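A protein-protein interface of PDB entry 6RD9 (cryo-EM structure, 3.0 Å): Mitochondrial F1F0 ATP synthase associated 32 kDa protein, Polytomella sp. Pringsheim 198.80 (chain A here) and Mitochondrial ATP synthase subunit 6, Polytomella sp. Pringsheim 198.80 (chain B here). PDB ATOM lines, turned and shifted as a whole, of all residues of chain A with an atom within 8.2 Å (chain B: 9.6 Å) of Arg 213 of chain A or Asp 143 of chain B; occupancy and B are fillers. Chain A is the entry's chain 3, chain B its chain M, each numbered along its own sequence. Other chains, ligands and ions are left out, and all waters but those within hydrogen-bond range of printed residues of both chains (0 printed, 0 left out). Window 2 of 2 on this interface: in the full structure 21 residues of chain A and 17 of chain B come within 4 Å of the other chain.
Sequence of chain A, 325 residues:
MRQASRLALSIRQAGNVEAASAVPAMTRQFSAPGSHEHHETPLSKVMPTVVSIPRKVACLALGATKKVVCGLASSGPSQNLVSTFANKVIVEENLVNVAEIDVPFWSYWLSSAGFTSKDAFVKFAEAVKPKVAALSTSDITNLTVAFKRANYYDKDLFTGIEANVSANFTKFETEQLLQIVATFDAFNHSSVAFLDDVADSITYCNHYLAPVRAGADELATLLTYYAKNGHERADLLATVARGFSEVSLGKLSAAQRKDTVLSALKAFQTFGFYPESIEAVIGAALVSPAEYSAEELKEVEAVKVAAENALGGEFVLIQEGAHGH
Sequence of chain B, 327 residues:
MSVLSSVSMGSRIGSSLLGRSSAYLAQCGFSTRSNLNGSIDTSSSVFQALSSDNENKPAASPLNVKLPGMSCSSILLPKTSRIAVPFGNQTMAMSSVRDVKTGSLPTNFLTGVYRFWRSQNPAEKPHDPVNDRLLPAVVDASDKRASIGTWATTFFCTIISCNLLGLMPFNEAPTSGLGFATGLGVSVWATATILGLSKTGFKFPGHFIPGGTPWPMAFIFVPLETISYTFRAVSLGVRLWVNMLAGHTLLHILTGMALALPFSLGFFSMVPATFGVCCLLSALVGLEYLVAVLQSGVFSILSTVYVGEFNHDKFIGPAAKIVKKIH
NH2 of Arg 213 of chain A lies within salt-bridge range of OD2 of Asp 143 of chain B.
OD2 of Asp 140 of chain B lies within salt-bridge range of NZ of Lys 144 of chain B. ND1 of His 207 of chain A is in hydrogen-bond range of N of Leu 209 of chain A, at 3.1 Å. The guanidinium group (NH2) of Arg 242 of chain A sits at hydrogen-bond distance from the backbone carbonyl oxygen (O) of Tyr 208 of chain A (3.3 Å).
Among the printed residues, pairs that only touch across the chains: Arg 242 of chain A with Pro 136 of chain B, Val 247 of chain A with Asp 140 of chain B, Arg 213 of chain A with Val 139 of chain B, Tyr 208 of chain A with Leu 135 of chain B, Val 212 of chain A with Pro 136 of chain B, Leu 209 of chain A with Leu 135 of chain B, Leu 209 of chain A with Val 139 of chain B, Val 247 of chain A with Pro 136 of chain B and Val 212 of chain A with Val 139 of chain B.
Of the printed residues of chain B, Leu 209 of chain A touches Leu 135 and Val 139. Of chain B, only Pro 136 (3.7 Å) and Val 139 (3.9 Å) come within 4 Å of Val 212 of chain A. Of chain B, only Val 139 and Asp 143 come within 4 Å of Arg 213 of chain A. Printed residues of chain A within 4 Å of Pro 136 of chain B: Val 212, Arg 242 and Val 247. Printed residues of chain A within 4 Å of Val 139 of chain B: Leu 209 (3.8 Å), Val 212 (3.9 Å) and Arg 213 (3.5 Å). Printed residues of chain A within 4 Å of Asp 140 of chain B: Val 247 (3.5 Å). Of the printed residues of chain A, Asp 143 of chain B touches Arg 213 (2.5 Å). The nearest printed residue of chain A that does not touch Leu 135 of chain B is Val 212 of chain A (4.7 Å).
Of the 19 printed residues of chain B, 5 touch a printed residue of chain A. Hydrophobic or aromatic side chains of chain A within 4 Å of the printed part of chain B: Tyr 208, Leu 209, Val 212 and Val 247.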
ATOM      1  N   THR A 174      21.622 -23.561 -17.030  1.00  0.00           N
ATOM      2  CA  THR A 174      21.536 -23.440 -18.477  1.00  0.00           C
ATOM      3  C   THR A 174      22.887 -23.663 -19.131  1.00  0.00           C
ATOM      4  O   THR A 174      22.957 -24.198 -20.234  1.00  0.00           O
ATOM      5  CB  THR A 174      20.967 -22.077 -18.837  1.00  0.00           C
ATOM      6  OG1 THR A 174      19.779 -21.867 -18.091  1.00  0.00           O
ATOM      7  CG2 THR A 174      20.624 -21.981 -20.278  1.00  0.00           C
ATOM      8  N   GLU A 175      23.969 -23.312 -18.450  1.00  0.00           N
ATOM      9  CA  GLU A 175      25.295 -23.690 -18.900  1.00  0.00           C
ATOM     10  C   GLU A 175      25.478 -25.194 -18.936  1.00  0.00           C
ATOM     11  O   GLU A 175      26.170 -25.699 -19.816  1.00  0.00           O
ATOM     12  CB  GLU A 175      26.328 -23.069 -17.969  1.00  0.00           C
ATOM     13  CG  GLU A 175      27.775 -23.275 -18.372  1.00  0.00           C
ATOM     14  CD  GLU A 175      28.743 -22.611 -17.423  1.00  0.00           C
ATOM     15  OE1 GLU A 175      28.280 -22.029 -16.423  1.00  0.00           O
ATOM     16  OE2 GLU A 175      29.965 -22.662 -17.680  1.00  0.00           O
ATOM     17  N   LEU A 178      22.575 -26.857 -21.648  1.00  0.00           N
ATOM     18  CA  LEU A 178      22.853 -26.657 -23.061  1.00  0.00           C
ATOM     19  C   LEU A 178      23.974 -27.545 -23.562  1.00  0.00           C
ATOM     20  O   LEU A 178      24.148 -27.674 -24.772  1.00  0.00           O
ATOM     21  CB  LEU A 178      23.209 -25.210 -23.340  1.00  0.00           C
ATOM     22  CG  LEU A 178      22.029 -24.268 -23.350  1.00  0.00           C
ATOM     23  CD1 LEU A 178      22.546 -22.896 -23.493  1.00  0.00           C
ATOM     24  CD2 LEU A 178      21.133 -24.590 -24.447  1.00  0.00           C
ATOM     25  N   HIS A 207      18.049 -18.437 -14.242  1.00  0.00           N
ATOM     26  CA  HIS A 207      17.957 -17.002 -14.436  1.00  0.00           C
ATOM     27  C   HIS A 207      17.574 -16.684 -15.864  1.00  0.00           C
ATOM     28  O   HIS A 207      17.965 -17.381 -16.791  1.00  0.00           O
ATOM     29  CB  HIS A 207      19.277 -16.339 -14.107  1.00  0.00           C
ATOM     30  CG  HIS A 207      19.158 -14.876 -13.854  1.00  0.00           C
ATOM     31  ND1 HIS A 207      19.169 -13.947 -14.861  1.00  0.00           N
ATOM     32  CD2 HIS A 207      18.989 -14.183 -12.713  1.00  0.00           C
ATOM     33  CE1 HIS A 207      19.028 -12.743 -14.352  1.00  0.00           C
ATOM     34  NE2 HIS A 207      18.909 -12.860 -13.049  1.00  0.00           N
ATOM     35  N   TYR A 208      16.770 -15.649 -16.044  1.00  0.00           N
ATOM     36  CA  TYR A 208      16.211 -15.413 -17.359  1.00  0.00           C
ATOM     37  C   TYR A 208      17.205 -14.806 -18.323  1.00  0.00           C
ATOM     38  O   TYR A 208      16.930 -14.772 -19.520  1.00  0.00           O
ATOM     39  CB  TYR A 208      14.967 -14.550 -17.233  1.00  0.00           C
ATOM     40  CG  TYR A 208      15.145 -13.078 -17.059  1.00  0.00           C
ATOM     41  CD1 TYR A 208      15.683 -12.553 -15.913  1.00  0.00           C
ATOM     42  CD2 TYR A 208      14.698 -12.216 -18.015  1.00  0.00           C
ATOM     43  CE1 TYR A 208      15.821 -11.208 -15.768  1.00  0.00           C
ATOM     44  CE2 TYR A 208      14.823 -10.889 -17.872  1.00  0.00           C
ATOM     45  CZ  TYR A 208      15.385 -10.390 -16.755  1.00  0.00           C
ATOM     46  OH  TYR A 208      15.488  -9.045 -16.648  1.00  0.00           O
ATOM     47  N   LEU A 209      18.358 -14.362 -17.846  1.00  0.00           N
ATOM     48  CA  LEU A 209      19.431 -13.897 -18.698  1.00  0.00           C
ATOM     49  C   LEU A 209      20.509 -14.929 -18.862  1.00  0.00           C
ATOM     50  O   LEU A 209      21.560 -14.615 -19.397  1.00  0.00           O
ATOM     51  CB  LEU A 209      20.055 -12.633 -18.141  1.00  0.00           C
ATOM     52  CG  LEU A 209      19.176 -11.447 -17.844  1.00  0.00           C
ATOM     53  CD1 LEU A 209      20.006 -10.459 -17.130  1.00  0.00           C
ATOM     54  CD2 LEU A 209      18.678 -10.875 -19.107  1.00  0.00           C
ATOM     55  N   ALA A 210      20.304 -16.116 -18.387  1.00  0.00           N
ATOM     56  CA  ALA A 210      21.227 -17.194 -18.674  1.00  0.00           C
ATOM     57  C   ALA A 210      21.300 -17.596 -20.147  1.00  0.00           C
ATOM     58  O   ALA A 210      22.341 -18.116 -20.550  1.00  0.00           O
ATOM     59  CB  ALA A 210      20.895 -18.410 -17.821  1.00  0.00           C
ATOM     60  N   PRO A 211      20.263 -17.426 -20.983  1.00  0.00           N
ATOM     61  CA  PRO A 211      20.504 -17.531 -22.424  1.00  0.00           C
ATOM     62  C   PRO A 211      21.410 -16.471 -23.003  1.00  0.00           C
ATOM     63  O   PRO A 211      22.044 -16.716 -24.030  1.00  0.00           O
ATOM     64  CB  PRO A 211      19.096 -17.414 -22.992  1.00  0.00           C
ATOM     65  CG  PRO A 211      18.316 -18.056 -22.039  1.00  0.00           C
ATOM     66  CD  PRO A 211      18.828 -17.670 -20.737  1.00  0.00           C
ATOM     67  N   VAL A 212      21.482 -15.293 -22.397  1.00  0.00           N
ATOM     68  CA  VAL A 212      22.315 -14.222 -22.921  1.00  0.00           C
ATOM     69  C   VAL A 212      23.793 -14.541 -22.734  1.00  0.00           C
ATOM     70  O   VAL A 212      24.639 -14.106 -23.519  1.00  0.00           O
ATOM     71  CB  VAL A 212      21.881 -12.922 -22.236  1.00  0.00           C
ATOM     72  CG1 VAL A 212      22.619 -11.776 -22.741  1.00  0.00           C
ATOM     73  CG2 VAL A 212      20.438 -12.695 -22.491  1.00  0.00           C
ATOM     74  N   ARG A 213      24.123 -15.342 -21.738  1.00  0.00           N
ATOM     75  CA  ARG A 213      25.479 -15.783 -21.481  1.00  0.00           C
ATOM     76  C   ARG A 213      25.838 -17.066 -22.194  1.00  0.00           C
ATOM     77  O   ARG A 213      26.837 -17.687 -21.837  1.00  0.00           O
ATOM     78  CB  ARG A 213      25.675 -15.995 -19.987  1.00  0.00           C
ATOM     79  CG  ARG A 213      25.919 -14.743 -19.217  1.00  0.00           C
ATOM     80  CD  ARG A 213      27.380 -14.418 -19.202  1.00  0.00           C
ATOM     81  NE  ARG A 213      27.639 -13.336 -18.285  1.00  0.00           N
ATOM     82  CZ  ARG A 213      27.550 -12.063 -18.613  1.00  0.00           C
ATOM     83  NH1 ARG A 213      27.784 -11.131 -17.713  1.00  0.00           N
ATOM     84  NH2 ARG A 213      27.242 -11.721 -19.849  1.00  0.00           N
ATOM     85  N   ALA A 214      25.066 -17.489 -23.184  1.00  0.00           N
ATOM     86  CA  ALA A 214      25.189 -18.852 -23.683  1.00  0.00           C
ATOM     87  C   ALA A 214      26.001 -18.964 -24.957  1.00  0.00           C
ATOM     88  O   ALA A 214      26.762 -19.919 -25.117  1.00  0.00           O
ATOM     89  CB  ALA A 214      23.812 -19.455 -23.927  1.00  0.00           C
ATOM     90  N   GLY A 215      25.851 -18.034 -25.879  1.00  0.00           N
ATOM     91  CA  GLY A 215      26.501 -18.211 -27.155  1.00  0.00           C
ATOM     92  C   GLY A 215      25.556 -18.919 -28.088  1.00  0.00           C
ATOM     93  O   GLY A 215      25.100 -20.023 -27.796  1.00  0.00           O
ATOM     94  N   ALA A 216      25.277 -18.299 -29.229  1.00  0.00           N
ATOM     95  CA  ALA A 216      24.102 -18.653 -29.999  1.00  0.00           C
ATOM     96  C   ALA A 216      24.244 -19.970 -30.738  1.00  0.00           C
ATOM     97  O   ALA A 216      23.255 -20.472 -31.270  1.00  0.00           O
ATOM     98  CB  ALA A 216      23.776 -17.531 -30.971  1.00  0.00           C
ATOM     99  N   GLU A 218      24.996 -22.734 -29.227  1.00  0.00           N
ATOM    100  CA  GLU A 218      24.428 -23.714 -28.321  1.00  0.00           C
ATOM    101  C   GLU A 218      22.935 -23.562 -28.189  1.00  0.00           C
ATOM    102  O   GLU A 218      22.243 -24.540 -27.914  1.00  0.00           O
ATOM    103  CB  GLU A 218      25.050 -23.590 -26.938  1.00  0.00           C
ATOM    104  CG  GLU A 218      26.362 -24.279 -26.785  1.00  0.00           C
ATOM    105  CD  GLU A 218      26.977 -24.018 -25.440  1.00  0.00           C
ATOM    106  OE1 GLU A 218      26.898 -22.868 -24.971  1.00  0.00           O
ATOM    107  OE2 GLU A 218      27.531 -24.962 -24.844  1.00  0.00           O
ATOM    108  N   LEU A 219      22.432 -22.347 -28.353  1.00  0.00           N
ATOM    109  CA  LEU A 219      21.000 -22.133 -28.284  1.00  0.00           C
ATOM    110  C   LEU A 219      20.300 -22.631 -29.529  1.00  0.00           C
ATOM    111  O   LEU A 219      19.146 -23.052 -29.458  1.00  0.00           O
ATOM    112  CB  LEU A 219      20.703 -20.665 -28.100  1.00  0.00           C
ATOM    113  CG  LEU A 219      21.279 -19.967 -26.897  1.00  0.00           C
ATOM    114  CD1 LEU A 219      20.979 -18.557 -27.126  1.00  0.00           C
ATOM    115  CD2 LEU A 219      20.601 -20.443 -25.658  1.00  0.00           C
ATOM    116  N   ARG A 242      15.908 -14.768 -26.151  1.00  0.00           N
ATOM    117  CA  ARG A 242      16.713 -13.694 -25.583  1.00  0.00           C
ATOM    118  C   ARG A 242      18.157 -13.832 -25.992  1.00  0.00           C
ATOM    119  O   ARG A 242      18.825 -12.840 -26.259  1.00  0.00           O
ATOM    120  CB  ARG A 242      16.629 -13.696 -24.070  1.00  0.00           C
ATOM    121  CG  ARG A 242      15.352 -13.203 -23.570  1.00  0.00           C
ATOM    122  CD  ARG A 242      15.156 -13.633 -22.175  1.00  0.00           C
ATOM    123  NE  ARG A 242      13.760 -13.441 -21.892  1.00  0.00           N
ATOM    124  CZ  ARG A 242      13.099 -14.146 -21.003  1.00  0.00           C
ATOM    125  NH1 ARG A 242      11.816 -13.927 -20.814  1.00  0.00           N
ATOM    126  NH2 ARG A 242      13.712 -15.119 -20.365  1.00  0.00           N
ATOM    127  N   GLY A 243      18.649 -15.043 -26.078  1.00  0.00           N
ATOM    128  CA  GLY A 243      20.056 -15.163 -26.317  1.00  0.00           C
ATOM    129  C   GLY A 243      20.499 -15.016 -27.741  1.00  0.00           C
ATOM    130  O   GLY A 243      21.641 -15.353 -28.048  1.00  0.00           O
ATOM    131  N   VAL A 247      25.057  -9.183 -30.350  1.00  0.00           N
ATOM    132  CA  VAL A 247      26.161  -9.494 -29.461  1.00  0.00           C
ATOM    133  C   VAL A 247      26.500 -10.967 -29.524  1.00  0.00           C
ATOM    134  O   VAL A 247      27.666 -11.344 -29.647  1.00  0.00           O
ATOM    135  CB  VAL A 247      25.798  -9.083 -28.033  1.00  0.00           C
ATOM    136  CG1 VAL A 247      26.989  -9.231 -27.151  1.00  0.00           C
ATOM    137  CG2 VAL A 247      25.239  -7.694 -28.006  1.00  0.00           C
ATOM    138  N   SER A 248      25.495 -11.821 -29.423  1.00  0.00           N
ATOM    139  CA  SER A 248      25.744 -13.245 -29.297  1.00  0.00           C
ATOM    140  C   SER A 248      26.148 -13.875 -30.612  1.00  0.00           C
ATOM    141  O   SER A 248      26.949 -14.813 -30.618  1.00  0.00           O
ATOM    142  CB  SER A 248      24.509 -13.928 -28.738  1.00  0.00           C
ATOM    143  OG  SER A 248      23.366 -13.521 -29.453  1.00  0.00           O
ATOM    144  N   LYS A 251      29.924 -12.861 -31.843  1.00  0.00           N
ATOM    145  CA  LYS A 251      31.035 -13.622 -31.297  1.00  0.00           C
ATOM    146  C   LYS A 251      31.275 -14.918 -32.045  1.00  0.00           C
ATOM    147  O   LYS A 251      32.161 -15.683 -31.658  1.00  0.00           O
ATOM    148  CB  LYS A 251      30.790 -13.921 -29.821  1.00  0.00           C
ATOM    149  CG  LYS A 251      30.624 -12.674 -29.001  1.00  0.00           C
ATOM    150  CD  LYS A 251      30.243 -12.977 -27.582  1.00  0.00           C
ATOM    151  CE  LYS A 251      29.930 -11.694 -26.847  1.00  0.00           C
ATOM    152  NZ  LYS A 251      29.681 -11.929 -25.414  1.00  0.00           N
ATOM    153  N   ALA B 123      24.970   3.815 -15.479  1.00  0.00           N
ATOM    154  CA  ALA B 123      24.814   3.364 -16.848  1.00  0.00           C
ATOM    155  C   ALA B 123      24.010   4.381 -17.632  1.00  0.00           C
ATOM    156  O   ALA B 123      23.192   5.114 -17.080  1.00  0.00           O
ATOM    157  CB  ALA B 123      24.127   2.006 -16.885  1.00  0.00           C
ATOM    158  N   LEU B 135      17.874  -6.517 -24.218  1.00  0.00           N
ATOM    159  CA  LEU B 135      18.465  -7.076 -23.009  1.00  0.00           C
ATOM    160  C   LEU B 135      19.853  -7.664 -23.195  1.00  0.00           C
ATOM    161  O   LEU B 135      20.653  -7.535 -22.258  1.00  0.00           O
ATOM    162  CB  LEU B 135      17.538  -8.121 -22.389  1.00  0.00           C
ATOM    163  CG  LEU B 135      16.584  -7.673 -21.303  1.00  0.00           C
ATOM    164  CD1 LEU B 135      15.955  -8.898 -20.741  1.00  0.00           C
ATOM    165  CD2 LEU B 135      17.291  -6.883 -20.248  1.00  0.00           C
ATOM    166  N   PRO B 136      20.221  -8.323 -24.300  1.00  0.00           N
ATOM    167  CA  PRO B 136      21.637  -8.659 -24.456  1.00  0.00           C
ATOM    168  C   PRO B 136      22.523  -7.479 -24.714  1.00  0.00           C
ATOM    169  O   PRO B 136      23.721  -7.574 -24.459  1.00  0.00           O
ATOM    170  CB  PRO B 136      21.642  -9.610 -25.645  1.00  0.00           C
ATOM    171  CG  PRO B 136      20.391 -10.179 -25.624  1.00  0.00           C
ATOM    172  CD  PRO B 136      19.440  -9.145 -25.235  1.00  0.00           C
ATOM    173  N   ALA B 137      21.998  -6.383 -25.235  1.00  0.00           N
ATOM    174  CA  ALA B 137      22.823  -5.207 -25.411  1.00  0.00           C
ATOM    175  C   ALA B 137      23.060  -4.505 -24.096  1.00  0.00           C
ATOM    176  O   ALA B 137      24.092  -3.861 -23.928  1.00  0.00           O
ATOM    177  CB  ALA B 137      22.174  -4.256 -26.400  1.00  0.00           C
ATOM    178  N   VAL B 138      22.125  -4.622 -23.160  1.00  0.00           N
ATOM    179  CA  VAL B 138      22.279  -4.053 -21.829  1.00  0.00           C
ATOM    180  C   VAL B 138      23.184  -4.923 -20.968  1.00  0.00           C
ATOM    181  O   VAL B 138      23.994  -4.417 -20.192  1.00  0.00           O
ATOM    182  CB  VAL B 138      20.884  -3.862 -21.223  1.00  0.00           C
ATOM    183  CG1 VAL B 138      20.944  -3.575 -19.779  1.00  0.00           C
ATOM    184  CG2 VAL B 138      20.206  -2.736 -21.914  1.00  0.00           C
ATOM    185  N   VAL B 139      23.084  -6.241 -21.104  1.00  0.00           N
ATOM    186  CA  VAL B 139      23.967  -7.146 -20.381  1.00  0.00           C
ATOM    187  C   VAL B 139      25.389  -7.041 -20.910  1.00  0.00           C
ATOM    188  O   VAL B 139      26.350  -7.078 -20.141  1.00  0.00           O
ATOM    189  CB  VAL B 139      23.406  -8.573 -20.471  1.00  0.00           C
ATOM    190  CG1 VAL B 139      24.408  -9.608 -20.088  1.00  0.00           C
ATOM    191  CG2 VAL B 139      22.232  -8.685 -19.593  1.00  0.00           C
ATOM    192  N   ASP B 140      25.551  -6.862 -22.220  1.00  0.00           N
ATOM    193  CA  ASP B 140      26.886  -6.660 -22.775  1.00  0.00           C
ATOM    194  C   ASP B 140      27.418  -5.276 -22.470  1.00  0.00           C
ATOM    195  O   ASP B 140      28.631  -5.082 -22.428  1.00  0.00           O
ATOM    196  CB  ASP B 140      26.879  -6.866 -24.277  1.00  0.00           C
ATOM    197  CG  ASP B 140      28.263  -6.897 -24.870  1.00  0.00           C
ATOM    198  OD1 ASP B 140      29.014  -7.854 -24.596  1.00  0.00           O
ATOM    199  OD2 ASP B 140      28.594  -5.969 -25.632  1.00  0.00           O
ATOM    200  N   ALA B 141      26.540  -4.301 -22.269  1.00  0.00           N
ATOM    201  CA  ALA B 141      27.000  -2.999 -21.820  1.00  0.00           C
ATOM    202  C   ALA B 141      27.518  -3.064 -20.400  1.00  0.00           C
ATOM    203  O   ALA B 141      28.408  -2.304 -20.032  1.00  0.00           O
ATOM    204  CB  ALA B 141      25.882  -1.977 -21.918  1.00  0.00           C
ATOM    205  N   SER B 142      26.969  -3.957 -19.584  1.00  0.00           N
ATOM    206  CA  SER B 142      27.471  -4.145 -18.232  1.00  0.00           C
ATOM    207  C   SER B 142      28.705  -5.020 -18.200  1.00  0.00           C
ATOM    208  O   SER B 142      29.475  -4.948 -17.247  1.00  0.00           O
ATOM    209  CB  SER B 142      26.403  -4.762 -17.357  1.00  0.00           C
ATOM    210  OG  SER B 142      25.293  -3.907 -17.281  1.00  0.00           O
ATOM    211  N   ASP B 143      28.902  -5.871 -19.196  1.00  0.00           N
ATOM    212  CA  ASP B 143      30.099  -6.692 -19.224  1.00  0.00           C
ATOM    213  C   ASP B 143      31.318  -5.918 -19.644  1.00  0.00           C
ATOM    214  O   ASP B 143      32.434  -6.395 -19.451  1.00  0.00           O
ATOM    215  CB  ASP B 143      29.950  -7.858 -20.187  1.00  0.00           C
ATOM    216  CG  ASP B 143      29.039  -8.919 -19.676  1.00  0.00           C
ATOM    217  OD1 ASP B 143      28.545  -8.789 -18.539  1.00  0.00           O
ATOM    218  OD2 ASP B 143      28.838  -9.909 -20.405  1.00  0.00           O
ATOM    219  N   LYS B 144      31.134  -4.770 -20.256  1.00  0.00           N
ATOM    220  CA  LYS B 144      32.235  -3.975 -20.739  1.00  0.00           C
ATOM    221  C   LYS B 144      32.529  -2.797 -19.839  1.00  0.00           C
ATOM    222  O   LYS B 144      33.545  -2.134 -20.024  1.00  0.00           O
ATOM    223  CB  LYS B 144      31.944  -3.514 -22.161  1.00  0.00           C
ATOM    224  CG  LYS B 144      31.913  -4.664 -23.144  1.00  0.00           C
ATOM    225  CD  LYS B 144      31.730  -4.201 -24.558  1.00  0.00           C
ATOM    226  CE  LYS B 144      30.470  -3.397 -24.703  1.00  0.00           C
ATOM    227  NZ  LYS B 144      30.196  -3.087 -26.120  1.00  0.00           N
ATOM    228  N   ARG B 145      31.671  -2.523 -18.873  1.00  0.00           N
ATOM    229  CA  ARG B 145      31.947  -1.504 -17.885  1.00  0.00           C
ATOM    230  C   ARG B 145      32.841  -2.072 -16.807  1.00  0.00           C
ATOM    231  O   ARG B 145      32.728  -3.239 -16.442  1.00  0.00           O
ATOM    232  CB  ARG B 145      30.658  -0.993 -17.276  1.00  0.00           C
ATOM    233  CG  ARG B 145      29.941  -0.096 -18.192  1.00  0.00           C
ATOM    234  CD  ARG B 145      28.570   0.222 -17.733  1.00  0.00           C
ATOM    235  NE  ARG B 145      28.598   1.251 -16.718  1.00  0.00           N
ATOM    236  CZ  ARG B 145      28.226   1.051 -15.468  1.00  0.00           C
ATOM    237  NH1 ARG B 145      28.287   2.036 -14.596  1.00  0.00           N
ATOM    238  NH2 ARG B 145      27.787  -0.139 -15.100  1.00  0.00           N
ATOM    239  N   ALA B 146      33.750  -1.248 -16.314  1.00  0.00           N
ATOM    240  CA  ALA B 146      34.614  -1.673 -15.240  1.00  0.00           C
ATOM    241  C   ALA B 146      33.818  -1.778 -13.956  1.00  0.00           C
ATOM    242  O   ALA B 146      32.786  -1.138 -13.780  1.00  0.00           O
ATOM    243  CB  ALA B 146      35.759  -0.692 -15.062  1.00  0.00           C
ATOM    244  N   SER B 147      34.310  -2.598 -13.043  1.00  0.00           N
ATOM    245  CA  SER B 147      33.652  -2.780 -11.760  1.00  0.00           C
ATOM    246  C   SER B 147      34.060  -1.674 -10.801  1.00  0.00           C
ATOM    247  O   SER B 147      34.615  -1.926  -9.753  1.00  0.00           O
ATOM    248  CB  SER B 147      34.002  -4.138 -11.184  1.00  0.00           C
ATOM    249  OG  SER B 147      33.342  -5.160 -11.879  1.00  0.00           O
ATOM    250  N   LEU B 195      42.881   0.141 -17.947  1.00  0.00           N
ATOM    251  CA  LEU B 195      41.548   0.130 -18.527  1.00  0.00           C
ATOM    252  C   LEU B 195      41.487   0.970 -19.791  1.00  0.00           C
ATOM    253  O   LEU B 195      40.903   0.550 -20.786  1.00  0.00           O
ATOM    254  CB  LEU B 195      40.541   0.629 -17.502  1.00  0.00           C
ATOM    255  CG  LEU B 195      39.092   0.772 -17.910  1.00  0.00           C
ATOM    256  CD1 LEU B 195      38.407  -0.520 -17.827  1.00  0.00           C
ATOM    257  CD2 LEU B 195      38.462   1.704 -16.978  1.00  0.00           C
ATOM    258  N   LYS B 199      41.103  -0.364 -24.095  1.00  0.00           N
ATOM    259  CA  LYS B 199      39.943   0.088 -24.914  1.00  0.00           C
ATOM    260  C   LYS B 199      40.333  -0.011 -26.391  1.00  0.00           C
ATOM    261  O   LYS B 199      39.434  -0.003 -27.254  1.00  0.00           O
ATOM    262  CB  LYS B 199      39.549   1.520 -24.539  1.00  0.00           C
ATOM    263  CG  LYS B 199      38.796   1.665 -23.224  1.00  0.00           C
ATOM    264  CD  LYS B 199      37.760   0.583 -23.003  1.00  0.00           C
ATOM    265  CE  LYS B 199      37.321   0.467 -21.559  1.00  0.00           C
ATOM    266  NZ  LYS B 199      37.353  -0.937 -21.086  1.00  0.00           N
ATOM    267  N   ASN B 311      35.573   4.498 -19.012  1.00  0.00           N
ATOM    268  CA  ASN B 311      34.489   3.545 -18.810  1.00  0.00           C
ATOM    269  C   ASN B 311      33.406   3.708 -19.859  1.00  0.00           C
ATOM    270  O   ASN B 311      32.225   3.715 -19.547  1.00  0.00           O
ATOM    271  CB  ASN B 311      33.918   3.736 -17.420  1.00  0.00           C
ATOM    272  CG  ASN B 311      33.365   2.496 -16.859  1.00  0.00           C
ATOM    273  OD1 ASN B 311      33.883   1.421 -17.096  1.00  0.00           O
ATOM    274  ND2 ASN B 311      32.316   2.624 -16.081  1.00  0.00           N
ATOM    275  N   ASP B 313      32.048   2.487 -23.762  1.00  0.00           N
ATOM    276  CA  ASP B 313      32.095   1.650 -24.944  1.00  0.00           C
ATOM    277  C   ASP B 313      30.850   1.874 -25.777  1.00  0.00           C
ATOM    278  O   ASP B 313      29.918   2.571 -25.374  1.00  0.00           O
ATOM    279  CB  ASP B 313      32.236   0.171 -24.602  1.00  0.00           C
ATOM    280  CG  ASP B 313      33.652  -0.221 -24.340  1.00  0.00           C
ATOM    281  OD1 ASP B 313      34.548   0.443 -24.887  1.00  0.00           O
ATOM    282  OD2 ASP B 313      33.890  -1.209 -23.626  1.00  0.00           O
ATOM    283  N   PHE B 315      27.422   1.120 -27.516  1.00  0.00           N
ATOM    284  CA  PHE B 315      26.240   0.298 -27.335  1.00  0.00           C
ATOM    285  C   PHE B 315      25.983  -0.482 -28.606  1.00  0.00           C
ATOM    286  O   PHE B 315      25.889   0.103 -29.685  1.00  0.00           O
ATOM    287  CB  PHE B 315      25.040   1.162 -26.991  1.00  0.00           C
ATOM    288  CG  PHE B 315      23.952   0.421 -26.303  1.00  0.00           C
ATOM    289  CD1 PHE B 315      24.045   0.130 -24.965  1.00  0.00           C
ATOM    290  CD2 PHE B 315      22.832   0.024 -26.988  1.00  0.00           C
ATOM    291  CE1 PHE B 315      23.049  -0.546 -24.332  1.00  0.00           C
ATOM    292  CE2 PHE B 315      21.840  -0.650 -26.356  1.00  0.00           C
ATOM    293  CZ  PHE B 315      21.947  -0.930 -25.031  1.00  0.00           C
